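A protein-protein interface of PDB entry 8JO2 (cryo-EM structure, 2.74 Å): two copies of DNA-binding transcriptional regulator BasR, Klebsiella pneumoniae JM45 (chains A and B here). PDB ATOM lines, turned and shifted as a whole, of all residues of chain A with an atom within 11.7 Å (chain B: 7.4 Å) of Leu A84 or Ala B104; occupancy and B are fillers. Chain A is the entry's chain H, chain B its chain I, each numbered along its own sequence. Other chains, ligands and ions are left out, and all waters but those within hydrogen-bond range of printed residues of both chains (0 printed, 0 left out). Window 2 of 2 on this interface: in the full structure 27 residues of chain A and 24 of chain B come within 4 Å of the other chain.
Of the 11 printed residues of chain B, 4 touch a printed residue of chain A.
Hydrophobic or aromatic side chains of chain B within 4 Å of the printed part of chain A: Ala B104 and Ala B110.
Among the printed residues, 6 pairs touch across the chains.
Among the printed residues, Asp or Glu carboxylates within 4 Å of a Lys or Arg side-chain nitrogen of the other chain: Arg A87 with Glu B107.
NH1 of Arg A87 is in salt-bridge range of OE1 of Glu B107, at 3.2 Å.
2 positions are printed for both chains.
Printed residues of chain B within 4 Å of Leu A84: Ala B104.
Ala B104 touches just one residue of chain A: Leu A84.
No residue of chain A comes within 4 Å of Pro B102.
No residue of chain A comes within 4 Å of Phe B103.
No residue of chain A comes within 4 Å of Leu B105.
Of chain A, only Ile A88 comes within 4 Å of Glu B106.
Of chain A, only Arg A87 and Ile A88 come within 4 Å of Glu B107.
No residue of chain A comes within 4 Å of Leu B108.
Of the printed residues of chain B, Leu A91 touches Ala B110 (3.7 Å).
Printed residues of chain B within 4 Å of Arg A87: Glu B107.
Of the printed residues of chain B, Ile A88 touches Glu B106, Glu B107 and Ala B110.
Of the printed residues of chain A, Ala B110 touches Ile A88 and Leu A91.
Leu A60 touches none of the printed residues of chain B.
Leu A52 touches none of the printed residues of chain B.
The side-chain carboxylate (OD1) of Asp A82 lies within salt-bridge range of the guanidinium group (NH2) of Arg A87, 3.2 Å away.
Leu A84 touches Ala B104.
CD1 of Ile A88 touches CB of Glu B106 (3.5 Å).
Ile A88 touches Glu B107 (CD1 to N, 3.7 Å).
Ala B110 touches Ile A88.
Ala B110 touches Leu A91.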
ATOM      1  N   LEU A  52     -27.069  -5.070 -25.875  1.00  0.00           N
ATOM      2  CA  LEU A  52     -27.156  -4.991 -27.357  1.00  0.00           C
ATOM      3  C   LEU A  52     -26.748  -6.330 -27.994  1.00  0.00           C
ATOM      4  O   LEU A  52     -27.088  -6.515 -29.179  1.00  0.00           O
ATOM      5  CB  LEU A  52     -26.283  -3.835 -27.856  1.00  0.00           C
ATOM      6  CG  LEU A  52     -26.685  -2.448 -27.354  1.00  0.00           C
ATOM      7  CD1 LEU A  52     -25.798  -1.368 -27.955  1.00  0.00           C
ATOM      8  CD2 LEU A  52     -28.148  -2.158 -27.646  1.00  0.00           C
ATOM      9  N   LEU A  60     -30.768  -2.050 -30.620  1.00  0.00           N
ATOM     10  CA  LEU A  60     -31.055  -0.665 -30.983  1.00  0.00           C
ATOM     11  C   LEU A  60     -32.424  -0.531 -31.641  1.00  0.00           C
ATOM     12  O   LEU A  60     -33.172   0.415 -31.357  1.00  0.00           O
ATOM     13  CB  LEU A  60     -29.962  -0.141 -31.909  1.00  0.00           C
ATOM     14  CG  LEU A  60     -28.758   0.483 -31.203  1.00  0.00           C
ATOM     15  CD1 LEU A  60     -27.642   0.747 -32.204  1.00  0.00           C
ATOM     16  CD2 LEU A  60     -29.121   1.747 -30.438  1.00  0.00           C
ATOM     17  N   ILE A  77     -27.798   0.724 -20.612  1.00  0.00           N
ATOM     18  CA  ILE A  77     -27.215  -0.205 -21.575  1.00  0.00           C
ATOM     19  C   ILE A  77     -25.994  -0.882 -20.973  1.00  0.00           C
ATOM     20  O   ILE A  77     -25.070  -0.217 -20.492  1.00  0.00           O
ATOM     21  CB  ILE A  77     -26.854   0.518 -22.877  1.00  0.00           C
ATOM     22  CG1 ILE A  77     -28.106   1.086 -23.528  1.00  0.00           C
ATOM     23  CG2 ILE A  77     -26.169  -0.432 -23.827  1.00  0.00           C
ATOM     24  CD1 ILE A  77     -29.059   0.029 -23.994  1.00  0.00           C
ATOM     25  N   THR A  79     -23.328  -3.169 -22.506  1.00  0.00           N
ATOM     26  CA  THR A  79     -22.815  -3.730 -23.747  1.00  0.00           C
ATOM     27  C   THR A  79     -21.313  -3.500 -23.836  1.00  0.00           C
ATOM     28  O   THR A  79     -20.715  -2.803 -23.012  1.00  0.00           O
ATOM     29  CB  THR A  79     -23.523  -3.131 -24.968  1.00  0.00           C
ATOM     30  OG1 THR A  79     -23.290  -3.964 -26.111  1.00  0.00           O
ATOM     31  CG2 THR A  79     -23.006  -1.739 -25.249  1.00  0.00           C
ATOM     32  N   ALA A  80     -20.705  -4.122 -24.847  1.00  0.00           N
ATOM     33  CA  ALA A  80     -19.272  -4.046 -25.087  1.00  0.00           C
ATOM     34  C   ALA A  80     -18.891  -3.065 -26.188  1.00  0.00           C
ATOM     35  O   ALA A  80     -17.698  -2.850 -26.413  1.00  0.00           O
ATOM     36  CB  ALA A  80     -18.727  -5.435 -25.432  1.00  0.00           C
ATOM     37  N   ARG A  81     -19.863  -2.463 -26.874  1.00  0.00           N
ATOM     38  CA  ARG A  81     -19.553  -1.612 -28.017  1.00  0.00           C
ATOM     39  C   ARG A  81     -19.013  -0.255 -27.586  1.00  0.00           C
ATOM     40  O   ARG A  81     -19.781   0.677 -27.328  1.00  0.00           O
ATOM     41  CB  ARG A  81     -20.785  -1.438 -28.905  1.00  0.00           C
ATOM     42  CG  ARG A  81     -21.236  -2.721 -29.580  1.00  0.00           C
ATOM     43  CD  ARG A  81     -22.439  -2.478 -30.467  1.00  0.00           C
ATOM     44  NE  ARG A  81     -23.050  -3.716 -30.939  1.00  0.00           N
ATOM     45  CZ  ARG A  81     -24.339  -3.848 -31.230  1.00  0.00           C
ATOM     46  NH1 ARG A  81     -24.808  -5.011 -31.650  1.00  0.00           N
ATOM     47  NH2 ARG A  81     -25.156  -2.811 -31.118  1.00  0.00           N
ATOM     48  N   ASP A  82     -17.690  -0.130 -27.537  1.00  0.00           N
ATOM     49  CA  ASP A  82     -17.014   1.025 -26.964  1.00  0.00           C
ATOM     50  C   ASP A  82     -16.739   2.106 -28.007  1.00  0.00           C
ATOM     51  O   ASP A  82     -16.278   3.194 -27.652  1.00  0.00           O
ATOM     52  CB  ASP A  82     -15.703   0.557 -26.313  1.00  0.00           C
ATOM     53  CG  ASP A  82     -15.012   1.629 -25.476  1.00  0.00           C
ATOM     54  OD1 ASP A  82     -15.490   2.773 -25.376  1.00  0.00           O
ATOM     55  OD2 ASP A  82     -13.952   1.308 -24.905  1.00  0.00           O
ATOM     56  N   THR A  83     -17.016   1.812 -29.282  1.00  0.00           N
ATOM     57  CA  THR A  83     -16.838   2.831 -30.356  1.00  0.00           C
ATOM     58  C   THR A  83     -17.609   4.094 -29.954  1.00  0.00           C
ATOM     59  O   THR A  83     -18.833   3.988 -29.774  1.00  0.00           O
ATOM     60  CB  THR A  83     -17.223   2.270 -31.737  1.00  0.00           C
ATOM     61  OG1 THR A  83     -18.585   1.837 -31.731  1.00  0.00           O
ATOM     62  CG2 THR A  83     -16.333   1.131 -32.190  1.00  0.00           C
ATOM     63  N   LEU A  84     -16.918   5.231 -29.822  1.00  0.00           N
ATOM     64  CA  LEU A  84     -17.562   6.500 -29.372  1.00  0.00           C
ATOM     65  C   LEU A  84     -18.850   6.760 -30.164  1.00  0.00           C
ATOM     66  O   LEU A  84     -19.872   7.062 -29.524  1.00  0.00           O
ATOM     67  CB  LEU A  84     -16.578   7.664 -29.533  1.00  0.00           C
ATOM     68  CG  LEU A  84     -17.018   9.002 -28.939  1.00  0.00           C
ATOM     69  CD1 LEU A  84     -15.820   9.783 -28.422  1.00  0.00           C
ATOM     70  CD2 LEU A  84     -17.787   9.821 -29.964  1.00  0.00           C
ATOM     71  N   GLU A  85     -18.791   6.652 -31.494  1.00  0.00           N
ATOM     72  CA  GLU A  85     -19.980   6.912 -32.351  1.00  0.00           C
ATOM     73  C   GLU A  85     -21.141   6.007 -31.928  1.00  0.00           C
ATOM     74  O   GLU A  85     -22.271   6.518 -31.860  1.00  0.00           O
ATOM     75  CB  GLU A  85     -19.626   6.696 -33.823  1.00  0.00           C
ATOM     76  CG  GLU A  85     -19.702   7.969 -34.645  1.00  0.00           C
ATOM     77  CD  GLU A  85     -18.804   9.094 -34.157  1.00  0.00           C
ATOM     78  OE1 GLU A  85     -19.335  10.082 -33.611  1.00  0.00           O
ATOM     79  OE2 GLU A  85     -17.574   8.981 -34.329  1.00  0.00           O
ATOM     80  N   ASP A  86     -20.874   4.725 -31.656  1.00  0.00           N
ATOM     81  CA  ASP A  86     -21.939   3.792 -31.299  1.00  0.00           C
ATOM     82  C   ASP A  86     -22.558   4.162 -29.955  1.00  0.00           C
ATOM     83  O   ASP A  86     -23.778   4.086 -29.779  1.00  0.00           O
ATOM     84  CB  ASP A  86     -21.390   2.364 -31.291  1.00  0.00           C
ATOM     85  CG  ASP A  86     -22.450   1.307 -31.006  1.00  0.00           C
ATOM     86  OD1 ASP A  86     -23.318   1.495 -30.131  1.00  0.00           O
ATOM     87  OD2 ASP A  86     -22.421   0.272 -31.701  1.00  0.00           O
ATOM     88  N   ARG A  87     -21.709   4.523 -28.988  1.00  0.00           N
ATOM     89  CA  ARG A  87     -22.221   4.962 -27.665  1.00  0.00           C
ATOM     90  C   ARG A  87     -23.194   6.120 -27.885  1.00  0.00           C
ATOM     91  O   ARG A  87     -24.323   6.036 -27.382  1.00  0.00           O
ATOM     92  CB  ARG A  87     -21.083   5.427 -26.753  1.00  0.00           C
ATOM     93  CG  ARG A  87     -19.832   4.562 -26.805  1.00  0.00           C
ATOM     94  CD  ARG A  87     -18.876   4.837 -25.662  1.00  0.00           C
ATOM     95  NE  ARG A  87     -18.472   6.234 -25.586  1.00  0.00           N
ATOM     96  CZ  ARG A  87     -17.224   6.668 -25.726  1.00  0.00           C
ATOM     97  NH1 ARG A  87     -16.963   7.960 -25.641  1.00  0.00           N
ATOM     98  NH2 ARG A  87     -16.243   5.814 -25.958  1.00  0.00           N
ATOM     99  N   ILE A  88     -22.764   7.150 -28.620  1.00  0.00           N
ATOM    100  CA  ILE A  88     -23.631   8.297 -28.877  1.00  0.00           C
ATOM    101  C   ILE A  88     -24.917   7.853 -29.559  1.00  0.00           C
ATOM    102  O   ILE A  88     -26.004   8.359 -29.267  1.00  0.00           O
ATOM    103  CB  ILE A  88     -22.896   9.356 -29.712  1.00  0.00           C
ATOM    104  CG1 ILE A  88     -21.703   9.896 -28.935  1.00  0.00           C
ATOM    105  CG2 ILE A  88     -23.834  10.486 -30.075  1.00  0.00           C
ATOM    106  CD1 ILE A  88     -20.798  10.736 -29.769  1.00  0.00           C
ATOM    107  N   SER A  89     -24.798   6.939 -30.521  1.00  0.00           N
ATOM    108  CA  SER A  89     -25.966   6.478 -31.263  1.00  0.00           C
ATOM    109  C   SER A  89     -26.967   5.811 -30.335  1.00  0.00           C
ATOM    110  O   SER A  89     -28.180   6.010 -30.457  1.00  0.00           O
ATOM    111  CB  SER A  89     -25.532   5.516 -32.366  1.00  0.00           C
ATOM    112  OG  SER A  89     -25.202   4.249 -31.825  1.00  0.00           O
ATOM    113  N   GLY A  90     -26.470   4.991 -29.413  1.00  0.00           N
ATOM    114  CA  GLY A  90     -27.346   4.394 -28.422  1.00  0.00           C
ATOM    115  C   GLY A  90     -28.021   5.436 -27.557  1.00  0.00           C
ATOM    116  O   GLY A  90     -29.233   5.389 -27.338  1.00  0.00           O
ATOM    117  N   LEU A  91     -27.243   6.400 -27.058  1.00  0.00           N
ATOM    118  CA  LEU A  91     -27.823   7.470 -26.252  1.00  0.00           C
ATOM    119  C   LEU A  91     -28.926   8.194 -27.003  1.00  0.00           C
ATOM    120  O   LEU A  91     -30.015   8.420 -26.465  1.00  0.00           O
ATOM    121  CB  LEU A  91     -26.752   8.472 -25.843  1.00  0.00           C
ATOM    122  CG  LEU A  91     -26.178   8.322 -24.444  1.00  0.00           C
ATOM    123  CD1 LEU A  91     -25.470   6.996 -24.323  1.00  0.00           C
ATOM    124  CD2 LEU A  91     -25.243   9.474 -24.162  1.00  0.00           C
ATOM    125  N   ASP A  92     -28.661   8.559 -28.253  1.00  0.00           N
ATOM    126  CA  ASP A  92     -29.632   9.316 -29.028  1.00  0.00           C
ATOM    127  C   ASP A  92     -30.853   8.472 -29.345  1.00  0.00           C
ATOM    128  O   ASP A  92     -31.972   8.993 -29.409  1.00  0.00           O
ATOM    129  CB  ASP A  92     -28.983   9.826 -30.311  1.00  0.00           C
ATOM    130  CG  ASP A  92     -27.937  10.890 -30.051  1.00  0.00           C
ATOM    131  OD1 ASP A  92     -28.068  11.621 -29.050  1.00  0.00           O
ATOM    132  OD2 ASP A  92     -26.978  10.991 -30.843  1.00  0.00           O
ATOM    133  N   THR A  93     -30.655   7.168 -29.542  1.00  0.00           N
ATOM    134  CA  THR A  93     -31.779   6.268 -29.753  1.00  0.00           C
ATOM    135  C   THR A  93     -32.698   6.239 -28.541  1.00  0.00           C
ATOM    136  O   THR A  93     -33.896   5.974 -28.678  1.00  0.00           O
ATOM    137  CB  THR A  93     -31.262   4.867 -30.072  1.00  0.00           C
ATOM    138  OG1 THR A  93     -30.255   4.958 -31.086  1.00  0.00           O
ATOM    139  CG2 THR A  93     -32.390   3.985 -30.581  1.00  0.00           C
ATOM    140  N   ALA A  95     -31.054   5.516 -25.048  1.00  0.00           N
ATOM    141  CA  ALA A  95     -30.319   4.979 -23.909  1.00  0.00           C
ATOM    142  C   ALA A  95     -30.060   6.106 -22.917  1.00  0.00           C
ATOM    143  O   ALA A  95     -29.375   7.078 -23.242  1.00  0.00           O
ATOM    144  CB  ALA A  95     -29.011   4.345 -24.369  1.00  0.00           C
ATOM    145  N   TYR A  98     -25.258   4.609 -20.233  1.00  0.00           N
ATOM    146  CA  TYR A  98     -24.594   3.661 -21.116  1.00  0.00           C
ATOM    147  C   TYR A  98     -23.391   3.096 -20.375  1.00  0.00           C
ATOM    148  O   TYR A  98     -22.402   3.806 -20.166  1.00  0.00           O
ATOM    149  CB  TYR A  98     -24.166   4.358 -22.401  1.00  0.00           C
ATOM    150  CG  TYR A  98     -23.525   3.459 -23.417  1.00  0.00           C
ATOM    151  CD1 TYR A  98     -24.296   2.601 -24.184  1.00  0.00           C
ATOM    152  CD2 TYR A  98     -22.158   3.437 -23.589  1.00  0.00           C
ATOM    153  CE1 TYR A  98     -23.728   1.773 -25.117  1.00  0.00           C
ATOM    154  CE2 TYR A  98     -21.580   2.601 -24.507  1.00  0.00           C
ATOM    155  CZ  TYR A  98     -22.367   1.774 -25.275  1.00  0.00           C
ATOM    156  OH  TYR A  98     -21.778   0.946 -26.199  1.00  0.00           O
ATOM    157  N   LEU A  99     -23.461   1.829 -19.987  1.00  0.00           N
ATOM    158  CA  LEU A  99     -22.404   1.194 -19.212  1.00  0.00           C
ATOM    159  C   LEU A  99     -21.602   0.273 -20.115  1.00  0.00           C
ATOM    160  O   LEU A  99     -22.176  -0.573 -20.809  1.00  0.00           O
ATOM    161  CB  LEU A  99     -22.975   0.419 -18.029  1.00  0.00           C
ATOM    162  CG  LEU A  99     -23.139   1.241 -16.758  1.00  0.00           C
ATOM    163  CD1 LEU A  99     -23.397   0.333 -15.575  1.00  0.00           C
ATOM    164  CD2 LEU A  99     -21.909   2.092 -16.520  1.00  0.00           C
ATOM    165  N   VAL A 100     -20.281   0.433 -20.101  1.00  0.00           N
ATOM    166  CA  VAL A 100     -19.389  -0.306 -20.981  1.00  0.00           C
ATOM    167  C   VAL A 100     -18.741  -1.440 -20.201  1.00  0.00           C
ATOM    168  O   VAL A 100     -18.300  -1.257 -19.060  1.00  0.00           O
ATOM    169  CB  VAL A 100     -18.335   0.619 -21.613  1.00  0.00           C
ATOM    170  CG1 VAL A 100     -19.010   1.804 -22.266  1.00  0.00           C
ATOM    171  CG2 VAL A 100     -17.342   1.107 -20.581  1.00  0.00           C
ATOM    172  N   LEU B  99     -18.659  11.993 -16.319  1.00  0.00           N
ATOM    173  CA  LEU B  99     -17.695  11.988 -17.416  1.00  0.00           C
ATOM    174  C   LEU B  99     -16.333  12.393 -16.869  1.00  0.00           C
ATOM    175  O   LEU B  99     -16.164  13.517 -16.383  1.00  0.00           O
ATOM    176  CB  LEU B  99     -18.125  12.926 -18.543  1.00  0.00           C
ATOM    177  CG  LEU B  99     -19.134  12.423 -19.582  1.00  0.00           C
ATOM    178  CD1 LEU B  99     -18.549  11.264 -20.369  1.00  0.00           C
ATOM    179  CD2 LEU B  99     -20.477  12.048 -18.985  1.00  0.00           C
ATOM    180  N   VAL B 100     -15.365  11.483 -16.948  1.00  0.00           N
ATOM    181  CA  VAL B 100     -14.018  11.786 -16.480  1.00  0.00           C
ATOM    182  C   VAL B 100     -13.258  12.565 -17.549  1.00  0.00           C
ATOM    183  O   VAL B 100     -13.570  12.512 -18.741  1.00  0.00           O
ATOM    184  CB  VAL B 100     -13.267  10.501 -16.090  1.00  0.00           C
ATOM    185  CG1 VAL B 100     -13.828   9.920 -14.809  1.00  0.00           C
ATOM    186  CG2 VAL B 100     -13.357   9.487 -17.208  1.00  0.00           C
ATOM    187  N   PRO B 102      -9.954  13.121 -19.855  1.00  0.00           N
ATOM    188  CA  PRO B 102     -10.627  13.950 -20.852  1.00  0.00           C
ATOM    189  C   PRO B 102     -11.843  13.243 -21.425  1.00  0.00           C
ATOM    190  O   PRO B 102     -12.014  12.038 -21.247  1.00  0.00           O
ATOM    191  CB  PRO B 102      -9.565  14.156 -21.931  1.00  0.00           C
ATOM    192  CG  PRO B 102      -8.560  13.090 -21.726  1.00  0.00           C
ATOM    193  CD  PRO B 102      -8.772  12.434 -20.399  1.00  0.00           C
ATOM    194  N   PHE B 103     -12.678  14.003 -22.116  1.00  0.00           N
ATOM    195  CA  PHE B 103     -13.858  13.489 -22.783  1.00  0.00           C
ATOM    196  C   PHE B 103     -13.831  13.954 -24.229  1.00  0.00           C
ATOM    197  O   PHE B 103     -13.047  14.826 -24.611  1.00  0.00           O
ATOM    198  CB  PHE B 103     -15.131  13.991 -22.105  1.00  0.00           C
ATOM    199  CG  PHE B 103     -15.291  15.476 -22.184  1.00  0.00           C
ATOM    200  CD1 PHE B 103     -14.761  16.288 -21.199  1.00  0.00           C
ATOM    201  CD2 PHE B 103     -15.974  16.061 -23.235  1.00  0.00           C
ATOM    202  CE1 PHE B 103     -14.897  17.657 -21.269  1.00  0.00           C
ATOM    203  CE2 PHE B 103     -16.117  17.427 -23.308  1.00  0.00           C
ATOM    204  CZ  PHE B 103     -15.579  18.227 -22.323  1.00  0.00           C
ATOM    205  N   ALA B 104     -14.711  13.380 -25.034  1.00  0.00           N
ATOM    206  CA  ALA B 104     -14.965  13.885 -26.372  1.00  0.00           C
ATOM    207  C   ALA B 104     -16.232  14.724 -26.349  1.00  0.00           C
ATOM    208  O   ALA B 104     -17.186  14.407 -25.634  1.00  0.00           O
ATOM    209  CB  ALA B 104     -15.106  12.751 -27.380  1.00  0.00           C
ATOM    210  N   LEU B 105     -16.228  15.800 -27.134  1.00  0.00           N
ATOM    211  CA  LEU B 105     -17.315  16.771 -27.075  1.00  0.00           C
ATOM    212  C   LEU B 105     -18.660  16.130 -27.388  1.00  0.00           C
ATOM    213  O   LEU B 105     -19.648  16.350 -26.675  1.00  0.00           O
ATOM    214  CB  LEU B 105     -17.033  17.922 -28.036  1.00  0.00           C
ATOM    215  CG  LEU B 105     -18.116  18.986 -27.959  1.00  0.00           C
ATOM    216  CD1 LEU B 105     -18.131  19.573 -26.568  1.00  0.00           C
ATOM    217  CD2 LEU B 105     -17.893  20.059 -29.009  1.00  0.00           C
ATOM    218  N   GLU B 106     -18.719  15.343 -28.460  1.00  0.00           N
ATOM    219  CA  GLU B 106     -19.988  14.770 -28.887  1.00  0.00           C
ATOM    220  C   GLU B 106     -20.561  13.855 -27.817  1.00  0.00           C
ATOM    221  O   GLU B 106     -21.776  13.835 -27.595  1.00  0.00           O
ATOM    222  CB  GLU B 106     -19.797  14.027 -30.206  1.00  0.00           C
ATOM    223  CG  GLU B 106     -19.047  14.840 -31.236  1.00  0.00           C
ATOM    224  CD  GLU B 106     -19.539  16.271 -31.302  1.00  0.00           C
ATOM    225  OE1 GLU B 106     -18.885  17.153 -30.706  1.00  0.00           O
ATOM    226  OE2 GLU B 106     -20.574  16.516 -31.956  1.00  0.00           O
ATOM    227  N   GLU B 107     -19.698  13.093 -27.146  1.00  0.00           N
ATOM    228  CA  GLU B 107     -20.130  12.314 -25.993  1.00  0.00           C
ATOM    229  C   GLU B 107     -20.875  13.185 -24.995  1.00  0.00           C
ATOM    230  O   GLU B 107     -21.985  12.850 -24.555  1.00  0.00           O
ATOM    231  CB  GLU B 107     -18.914  11.664 -25.330  1.00  0.00           C
ATOM    232  CG  GLU B 107     -19.220  10.787 -24.124  1.00  0.00           C
ATOM    233  CD  GLU B 107     -20.032   9.559 -24.459  1.00  0.00           C
ATOM    234  OE1 GLU B 107     -19.968   9.098 -25.613  1.00  0.00           O
ATOM    235  OE2 GLU B 107     -20.720   9.041 -23.556  1.00  0.00           O
ATOM    236  N   LEU B 108     -20.277  14.312 -24.626  1.00  0.00           N
ATOM    237  CA  LEU B 108     -20.869  15.148 -23.594  1.00  0.00           C
ATOM    238  C   LEU B 108     -22.197  15.730 -24.055  1.00  0.00           C
ATOM    239  O   LEU B 108     -23.177  15.731 -23.303  1.00  0.00           O
ATOM    240  CB  LEU B 108     -19.880  16.236 -23.189  1.00  0.00           C
ATOM    241  CG  LEU B 108     -20.243  17.136 -22.012  1.00  0.00           C
ATOM    242  CD1 LEU B 108     -19.039  17.232 -21.119  1.00  0.00           C
ATOM    243  CD2 LEU B 108     -20.605  18.509 -22.508  1.00  0.00           C
ATOM    244  N   ASN B 109     -22.237  16.212 -25.300  1.00  0.00           N
ATOM    245  CA  ASN B 109     -23.488  16.802 -25.848  1.00  0.00           C
ATOM    246  C   ASN B 109     -24.584  15.729 -25.878  1.00  0.00           C
ATOM    247  O   ASN B 109     -25.748  16.088 -25.638  1.00  0.00           O
ATOM    248  CB  ASN B 109     -23.255  17.455 -27.212  1.00  0.00           C
ATOM    249  CG  ASN B 109     -22.187  18.528 -27.197  1.00  0.00           C
ATOM    250  OD1 ASN B 109     -21.872  19.093 -26.151  1.00  0.00           O
ATOM    251  ND2 ASN B 109     -21.625  18.818 -28.359  1.00  0.00           N
ATOM    252  N   ALA B 110     -24.235  14.474 -26.187  1.00  0.00           N
ATOM    253  CA  ALA B 110     -25.205  13.383 -26.176  1.00  0.00           C
ATOM    254  C   ALA B 110     -25.748  13.139 -24.775  1.00  0.00           C
ATOM    255  O   ALA B 110     -26.964  13.012 -24.578  1.00  0.00           O
ATOM    256  CB  ALA B 110     -24.567  12.110 -26.730  1.00  0.00           C
